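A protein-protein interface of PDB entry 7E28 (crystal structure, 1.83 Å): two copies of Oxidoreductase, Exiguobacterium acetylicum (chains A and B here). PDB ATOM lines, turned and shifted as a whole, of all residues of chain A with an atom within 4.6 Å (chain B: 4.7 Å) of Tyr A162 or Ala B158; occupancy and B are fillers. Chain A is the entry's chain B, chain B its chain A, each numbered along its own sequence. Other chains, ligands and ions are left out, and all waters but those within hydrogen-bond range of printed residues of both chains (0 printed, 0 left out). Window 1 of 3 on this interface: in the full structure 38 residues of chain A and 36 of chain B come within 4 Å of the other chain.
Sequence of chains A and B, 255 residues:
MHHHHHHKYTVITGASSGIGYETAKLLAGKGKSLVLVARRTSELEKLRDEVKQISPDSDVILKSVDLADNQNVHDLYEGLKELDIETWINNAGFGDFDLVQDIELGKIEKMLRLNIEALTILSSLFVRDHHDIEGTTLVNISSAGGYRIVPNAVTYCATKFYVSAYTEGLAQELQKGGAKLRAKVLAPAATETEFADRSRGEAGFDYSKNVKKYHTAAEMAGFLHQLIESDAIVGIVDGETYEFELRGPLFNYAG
Tyr A162 touches just these residues of chain B: Leu B112 (3.6 Å), Ile B116 (3.6 Å), Thr B155 (3.7 Å), Ala B158 (3.2 Å) and Thr B159 (3.6 Å).
Of chain A, only Tyr A162 and Tyr A166 come within 4 Å of Ala B158.
Of the printed residues of chain B, Thr A159 touches Tyr B162.
Of the printed residues of chain A, Tyr B162 touches Ile A116, Ala A158 and Thr A159.
Of the printed residues of chain B, Ile A116 touches Tyr B162 (3.8 Å).
Printed residues of chain B within 4 Å of Thr A120: Leu B112.
Val A163 touches none of the printed residues of chain B.
Phe A161 touches none of the printed residues of chain B.
The nearest residue of chain B that does not touch Tyr A162 is Tyr B162 (4.2 Å).
OG1 of Thr B159 is in hydrogen-bond range of O of Tyr B156, at 2.6 Å.
The backbone carbonyl oxygen (O) of Ile A116 is in hydrogen-bond range of the side-chain hydroxyl (OG1) of Thr A120.
The side-chain hydroxyl of Thr A120 sits at hydrogen-bond distance from the side-chain hydroxyl of Tyr A162 (2.6 Å).
Ile A116 touches Tyr B162, and with the chains exchanged Tyr A162 touches Ile B116.
Ala A158 touches Tyr B162, and with the chains exchanged Tyr A162 touches Ala B158.
Thr A159 touches Tyr B162, and with the chains exchanged Tyr A162 touches Thr B159.
6 positions are printed for both chains.
Of the 13 pairs that touch across the chains among the printed residues, 6 have their exchanged pair printed and touching as well.
Of the 11 printed residues of chain B, 8 touch a printed residue of chain A.
Hydrophobic or aromatic side chains of chain B within 4 Å of the printed part of chain A: Leu B112, Ile B116, Val B154, Ala B158, Phe B161 and Tyr B162.
Of the 11 printed residues of chain A, 7 touch a printed residue of chain B.
Hydrophobic or aromatic side chains of chain A that line the printed part of chain B: Ile A116, Ala A158, Tyr A162, Ala A165 and Tyr A166.
CD1 of Ile A116 touches CD1 of Tyr B162 (3.8 Å).
Thr A120 touches Leu B112 (CB to CD1, 3.9 Å).
Tyr B162 touches Thr A159.
CD2 of Leu B112 touches OH of Tyr A162, at 3.6 Å.
CD2 of Tyr A162 touches CD1 of Ile B116, at 3.6 Å.
Thr B155 touches Tyr A162.
Tyr A162 touches Thr B159.
CG of Phe B161 touches CB of Ala A165, at 3.5 Å.
Tyr A166 touches Thr B155 (CE1 to OG1, 3.6 Å).
Tyr A166 touches Ala B158.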
ATOM      1  N   ILE A 116     -10.922   1.456 -24.599  1.00  0.00           N
ATOM      2  CA  ILE A 116      -9.792   1.707 -23.705  1.00  0.00           C
ATOM      3  C   ILE A 116     -10.262   1.901 -22.272  1.00  0.00           C
ATOM      4  O   ILE A 116      -9.800   1.206 -21.359  1.00  0.00           O
ATOM      5  CB  ILE A 116      -8.955   2.924 -24.173  1.00  0.00           C
ATOM      6  CG1 ILE A 116      -8.288   2.623 -25.519  1.00  0.00           C
ATOM      7  CG2 ILE A 116      -7.914   3.309 -23.096  1.00  0.00           C
ATOM      8  CD1 ILE A 116      -7.687   3.873 -26.229  1.00  0.00           C
ATOM      9  N   THR A 120     -10.050  -0.778 -19.348  1.00  0.00           N
ATOM     10  CA  THR A 120      -9.050  -0.528 -18.313  1.00  0.00           C
ATOM     11  C   THR A 120      -9.676  -0.575 -16.923  1.00  0.00           C
ATOM     12  O   THR A 120      -9.079  -1.109 -15.975  1.00  0.00           O
ATOM     13  CB  THR A 120      -8.370   0.825 -18.557  1.00  0.00           C
ATOM     14  OG1 THR A 120      -7.667   0.775 -19.801  1.00  0.00           O
ATOM     15  CG2 THR A 120      -7.381   1.135 -17.463  1.00  0.00           C
ATOM     16  N   ALA A 158      -4.605   2.342 -32.881  1.00  0.00           N
ATOM     17  CA  ALA A 158      -3.980   2.868 -31.677  1.00  0.00           C
ATOM     18  C   ALA A 158      -4.682   2.359 -30.410  1.00  0.00           C
ATOM     19  O   ALA A 158      -4.004   1.996 -29.439  1.00  0.00           O
ATOM     20  CB  ALA A 158      -3.942   4.387 -31.721  1.00  0.00           C
ATOM     21  N   THR A 159      -6.033   2.300 -30.399  1.00  0.00           N
ATOM     22  CA  THR A 159      -6.724   1.717 -29.240  1.00  0.00           C
ATOM     23  C   THR A 159      -6.290   0.278 -29.020  1.00  0.00           C
ATOM     24  O   THR A 159      -6.162  -0.174 -27.874  1.00  0.00           O
ATOM     25  CB  THR A 159      -8.267   1.754 -29.364  1.00  0.00           C
ATOM     26  OG1 THR A 159      -8.754   0.725 -30.248  1.00  0.00           O
ATOM     27  CG2 THR A 159      -8.791   3.106 -29.796  1.00  0.00           C
ATOM     28  N   LYS A 160      -6.063  -0.467 -30.105  1.00  0.00           N
ATOM     29  CA  LYS A 160      -5.684  -1.863 -29.942  1.00  0.00           C
ATOM     30  C   LYS A 160      -4.209  -2.024 -29.580  1.00  0.00           C
ATOM     31  O   LYS A 160      -3.843  -3.028 -28.956  1.00  0.00           O
ATOM     32  CB  LYS A 160      -6.053  -2.644 -31.206  1.00  0.00           C
ATOM     33  CG  LYS A 160      -7.563  -2.802 -31.384  1.00  0.00           C
ATOM     34  CD  LYS A 160      -8.290  -3.118 -30.048  1.00  0.00           C
ATOM     35  CE  LYS A 160      -9.659  -3.706 -30.344  1.00  0.00           C
ATOM     36  NZ  LYS A 160     -10.424  -4.111 -29.118  1.00  0.00           N
ATOM     37  N   PHE A 161      -3.347  -1.070 -29.956  1.00  0.00           N
ATOM     38  CA  PHE A 161      -1.997  -1.052 -29.391  1.00  0.00           C
ATOM     39  C   PHE A 161      -2.064  -0.831 -27.885  1.00  0.00           C
ATOM     40  O   PHE A 161      -1.360  -1.498 -27.109  1.00  0.00           O
ATOM     41  CB  PHE A 161      -1.147   0.037 -30.054  1.00  0.00           C
ATOM     42  CG  PHE A 161      -0.399  -0.433 -31.261  1.00  0.00           C
ATOM     43  CD1 PHE A 161      -1.063  -0.653 -32.463  1.00  0.00           C
ATOM     44  CD2 PHE A 161       0.981  -0.635 -31.207  1.00  0.00           C
ATOM     45  CE1 PHE A 161      -0.381  -1.094 -33.576  1.00  0.00           C
ATOM     46  CE2 PHE A 161       1.671  -1.059 -32.320  1.00  0.00           C
ATOM     47  CZ  PHE A 161       0.995  -1.290 -33.515  1.00  0.00           C
ATOM     48  N   TYR A 162      -2.925   0.096 -27.450  1.00  0.00           N
ATOM     49  CA  TYR A 162      -3.174   0.254 -26.022  1.00  0.00           C
ATOM     50  C   TYR A 162      -3.553  -1.087 -25.405  1.00  0.00           C
ATOM     51  O   TYR A 162      -2.926  -1.539 -24.446  1.00  0.00           O
ATOM     52  CB  TYR A 162      -4.274   1.300 -25.750  1.00  0.00           C
ATOM     53  CG  TYR A 162      -4.536   1.452 -24.251  1.00  0.00           C
ATOM     54  CD1 TYR A 162      -5.317   0.516 -23.560  1.00  0.00           C
ATOM     55  CD2 TYR A 162      -3.967   2.494 -23.516  1.00  0.00           C
ATOM     56  CE1 TYR A 162      -5.530   0.608 -22.185  1.00  0.00           C
ATOM     57  CE2 TYR A 162      -4.187   2.611 -22.142  1.00  0.00           C
ATOM     58  CZ  TYR A 162      -4.980   1.641 -21.486  1.00  0.00           C
ATOM     59  OH  TYR A 162      -5.211   1.707 -20.123  1.00  0.00           O
ATOM     60  N   VAL A 163      -4.584  -1.738 -25.949  1.00  0.00           N
ATOM     61  CA  VAL A 163      -5.062  -2.981 -25.346  1.00  0.00           C
ATOM     62  C   VAL A 163      -3.948  -4.017 -25.287  1.00  0.00           C
ATOM     63  O   VAL A 163      -3.747  -4.675 -24.256  1.00  0.00           O
ATOM     64  CB  VAL A 163      -6.287  -3.529 -26.103  1.00  0.00           C
ATOM     65  CG1 VAL A 163      -6.706  -4.898 -25.522  1.00  0.00           C
ATOM     66  CG2 VAL A 163      -7.445  -2.537 -26.033  1.00  0.00           C
ATOM     67  N   SER A 164      -3.222  -4.196 -26.394  1.00  0.00           N
ATOM     68  CA  SER A 164      -2.170  -5.205 -26.428  1.00  0.00           C
ATOM     69  C   SER A 164      -1.065  -4.900 -25.432  1.00  0.00           C
ATOM     70  O   SER A 164      -0.656  -5.792 -24.678  1.00  0.00           O
ATOM     71  CB  SER A 164      -1.599  -5.349 -27.834  1.00  0.00           C
ATOM     72  OG  SER A 164      -2.598  -5.828 -28.712  1.00  0.00           O
ATOM     73  N   ALA A 165      -0.569  -3.653 -25.420  1.00  0.00           N
ATOM     74  CA  ALA A 165       0.480  -3.272 -24.479  1.00  0.00           C
ATOM     75  C   ALA A 165       0.003  -3.392 -23.036  1.00  0.00           C
ATOM     76  O   ALA A 165       0.724  -3.915 -22.181  1.00  0.00           O
ATOM     77  CB  ALA A 165       0.968  -1.846 -24.767  1.00  0.00           C
ATOM     78  N   TYR A 166      -1.198  -2.885 -22.744  1.00  0.00           N
ATOM     79  CA  TYR A 166      -1.759  -2.995 -21.400  1.00  0.00           C
ATOM     80  C   TYR A 166      -1.833  -4.453 -20.953  1.00  0.00           C
ATOM     81  O   TYR A 166      -1.432  -4.810 -19.827  1.00  0.00           O
ATOM     82  CB  TYR A 166      -3.156  -2.363 -21.375  1.00  0.00           C
ATOM     83  CG  TYR A 166      -3.833  -2.471 -20.037  1.00  0.00           C
ATOM     84  CD1 TYR A 166      -3.546  -1.559 -19.032  1.00  0.00           C
ATOM     85  CD2 TYR A 166      -4.750  -3.493 -19.768  1.00  0.00           C
ATOM     86  CE1 TYR A 166      -4.138  -1.648 -17.803  1.00  0.00           C
ATOM     87  CE2 TYR A 166      -5.352  -3.590 -18.532  1.00  0.00           C
ATOM     88  CZ  TYR A 166      -5.032  -2.657 -17.550  1.00  0.00           C
ATOM     89  OH  TYR A 166      -5.599  -2.706 -16.301  1.00  0.00           O
ATOM     90  N   LEU B 112      -6.163   8.585 -18.519  1.00  0.00           N
ATOM     91  CA  LEU B 112      -6.694   8.204 -19.827  1.00  0.00           C
ATOM     92  C   LEU B 112      -7.337   9.392 -20.540  1.00  0.00           C
ATOM     93  O   LEU B 112      -7.226   9.528 -21.766  1.00  0.00           O
ATOM     94  CB  LEU B 112      -7.708   7.067 -19.667  1.00  0.00           C
ATOM     95  CG  LEU B 112      -7.103   5.774 -19.095  1.00  0.00           C
ATOM     96  CD1 LEU B 112      -8.205   4.744 -18.937  1.00  0.00           C
ATOM     97  CD2 LEU B 112      -5.968   5.208 -19.941  1.00  0.00           C
ATOM     98  N   ILE B 116      -4.707  10.378 -23.542  1.00  0.00           N
ATOM     99  CA  ILE B 116      -5.302   9.767 -24.733  1.00  0.00           C
ATOM    100  C   ILE B 116      -6.418  10.629 -25.321  1.00  0.00           C
ATOM    101  O   ILE B 116      -6.358  11.027 -26.492  1.00  0.00           O
ATOM    102  CB  ILE B 116      -5.799   8.337 -24.444  1.00  0.00           C
ATOM    103  CG1 ILE B 116      -4.609   7.430 -24.074  1.00  0.00           C
ATOM    104  CG2 ILE B 116      -6.560   7.810 -25.664  1.00  0.00           C
ATOM    105  CD1 ILE B 116      -4.981   5.987 -23.787  1.00  0.00           C
ATOM    106  N   VAL B 154       2.429  -0.112 -15.954  1.00  0.00           N
ATOM    107  CA  VAL B 154       1.761  -0.773 -17.075  1.00  0.00           C
ATOM    108  C   VAL B 154       0.732   0.158 -17.712  1.00  0.00           C
ATOM    109  O   VAL B 154       0.632   0.250 -18.942  1.00  0.00           O
ATOM    110  CB  VAL B 154       1.114  -2.096 -16.637  1.00  0.00           C
ATOM    111  CG1 VAL B 154       0.276  -2.672 -17.786  1.00  0.00           C
ATOM    112  CG2 VAL B 154       2.192  -3.109 -16.182  1.00  0.00           C
ATOM    113  N   THR B 155      -0.057   0.853 -16.891  1.00  0.00           N
ATOM    114  CA  THR B 155      -1.143   1.636 -17.468  1.00  0.00           C
ATOM    115  C   THR B 155      -0.599   2.877 -18.161  1.00  0.00           C
ATOM    116  O   THR B 155      -1.004   3.197 -19.289  1.00  0.00           O
ATOM    117  CB  THR B 155      -2.175   2.002 -16.398  1.00  0.00           C
ATOM    118  OG1 THR B 155      -2.614   0.814 -15.714  1.00  0.00           O
ATOM    119  CG2 THR B 155      -3.378   2.667 -17.051  1.00  0.00           C
ATOM    120  N   TYR B 156       0.320   3.586 -17.499  1.00  0.00           N
ATOM    121  CA  TYR B 156       0.979   4.727 -18.121  1.00  0.00           C
ATOM    122  C   TYR B 156       1.631   4.324 -19.437  1.00  0.00           C
ATOM    123  O   TYR B 156       1.486   5.016 -20.454  1.00  0.00           O
ATOM    124  CB  TYR B 156       2.031   5.336 -17.185  1.00  0.00           C
ATOM    125  CG  TYR B 156       2.845   6.424 -17.891  1.00  0.00           C
ATOM    126  CD1 TYR B 156       2.252   7.635 -18.253  1.00  0.00           C
ATOM    127  CD2 TYR B 156       4.191   6.227 -18.212  1.00  0.00           C
ATOM    128  CE1 TYR B 156       2.978   8.638 -18.894  1.00  0.00           C
ATOM    129  CE2 TYR B 156       4.924   7.223 -18.864  1.00  0.00           C
ATOM    130  CZ  TYR B 156       4.311   8.424 -19.192  1.00  0.00           C
ATOM    131  OH  TYR B 156       5.031   9.416 -19.840  1.00  0.00           O
ATOM    132  N   CYS B 157       2.382   3.214 -19.429  1.00  0.00           N
ATOM    133  CA  CYS B 157       3.031   2.777 -20.658  1.00  0.00           C
ATOM    134  C   CYS B 157       2.003   2.511 -21.746  1.00  0.00           C
ATOM    135  O   CYS B 157       2.203   2.898 -22.908  1.00  0.00           O
ATOM    136  CB  CYS B 157       3.900   1.552 -20.373  1.00  0.00           C
ATOM    137  SG  CYS B 157       5.484   2.014 -19.494  1.00  0.00           S
ATOM    138  N   ALA B 158       0.886   1.874 -21.373  1.00  0.00           N
ATOM    139  CA  ALA B 158      -0.165   1.590 -22.338  1.00  0.00           C
ATOM    140  C   ALA B 158      -0.657   2.863 -23.026  1.00  0.00           C
ATOM    141  O   ALA B 158      -0.878   2.873 -24.243  1.00  0.00           O
ATOM    142  CB  ALA B 158      -1.316   0.869 -21.647  1.00  0.00           C
ATOM    143  N   THR B 159      -0.848   3.952 -22.263  1.00  0.00           N
ATOM    144  CA  THR B 159      -1.275   5.205 -22.888  1.00  0.00           C
ATOM    145  C   THR B 159      -0.230   5.713 -23.873  1.00  0.00           C
ATOM    146  O   THR B 159      -0.573   6.317 -24.901  1.00  0.00           O
ATOM    147  CB  THR B 159      -1.544   6.291 -21.836  1.00  0.00           C
ATOM    148  OG1 THR B 159      -0.304   6.765 -21.276  1.00  0.00           O
ATOM    149  CG2 THR B 159      -2.408   5.760 -20.723  1.00  0.00           C
ATOM    150  N   LYS B 160       1.050   5.487 -23.574  1.00  0.00           N
ATOM    151  CA  LYS B 160       2.103   5.970 -24.453  1.00  0.00           C
ATOM    152  C   LYS B 160       2.298   5.045 -25.646  1.00  0.00           C
ATOM    153  O   LYS B 160       2.681   5.520 -26.721  1.00  0.00           O
ATOM    154  CB  LYS B 160       3.392   6.185 -23.661  1.00  0.00           C
ATOM    155  CG  LYS B 160       3.277   7.273 -22.590  1.00  0.00           C
ATOM    156  CD  LYS B 160       2.590   8.511 -23.148  1.00  0.00           C
ATOM    157  CE  LYS B 160       2.789   9.728 -22.256  1.00  0.00           C
ATOM    158  NZ  LYS B 160       2.445  11.012 -22.952  1.00  0.00           N
ATOM    159  N   PHE B 161       2.008   3.742 -25.514  1.00  0.00           N
ATOM    160  CA  PHE B 161       1.909   2.928 -26.727  1.00  0.00           C
ATOM    161  C   PHE B 161       0.799   3.458 -27.639  1.00  0.00           C
ATOM    162  O   PHE B 161       0.929   3.441 -28.874  1.00  0.00           O
ATOM    163  CB  PHE B 161       1.669   1.457 -26.388  1.00  0.00           C
ATOM    164  CG  PHE B 161       2.943   0.662 -26.211  1.00  0.00           C
ATOM    165  CD1 PHE B 161       3.734   0.832 -25.067  1.00  0.00           C
ATOM    166  CD2 PHE B 161       3.356  -0.251 -27.182  1.00  0.00           C
ATOM    167  CE1 PHE B 161       4.910   0.123 -24.905  1.00  0.00           C
ATOM    168  CE2 PHE B 161       4.531  -0.965 -27.024  1.00  0.00           C
ATOM    169  CZ  PHE B 161       5.311  -0.781 -25.876  1.00  0.00           C
ATOM    170  N   TYR B 162      -0.310   3.916 -27.044  1.00  0.00           N
ATOM    171  CA  TYR B 162      -1.366   4.541 -27.833  1.00  0.00           C
ATOM    172  C   TYR B 162      -0.831   5.776 -28.536  1.00  0.00           C
ATOM    173  O   TYR B 162      -1.033   5.958 -29.743  1.00  0.00           O
ATOM    174  CB  TYR B 162      -2.576   4.926 -26.958  1.00  0.00           C
ATOM    175  CG  TYR B 162      -3.660   5.645 -27.766  1.00  0.00           C
ATOM    176  CD1 TYR B 162      -4.733   4.948 -28.337  1.00  0.00           C
ATOM    177  CD2 TYR B 162      -3.562   7.018 -28.034  1.00  0.00           C
ATOM    178  CE1 TYR B 162      -5.693   5.617 -29.118  1.00  0.00           C
ATOM    179  CE2 TYR B 162      -4.510   7.680 -28.804  1.00  0.00           C
ATOM    180  CZ  TYR B 162      -5.561   6.980 -29.349  1.00  0.00           C
ATOM    181  OH  TYR B 162      -6.492   7.664 -30.130  1.00  0.00           O
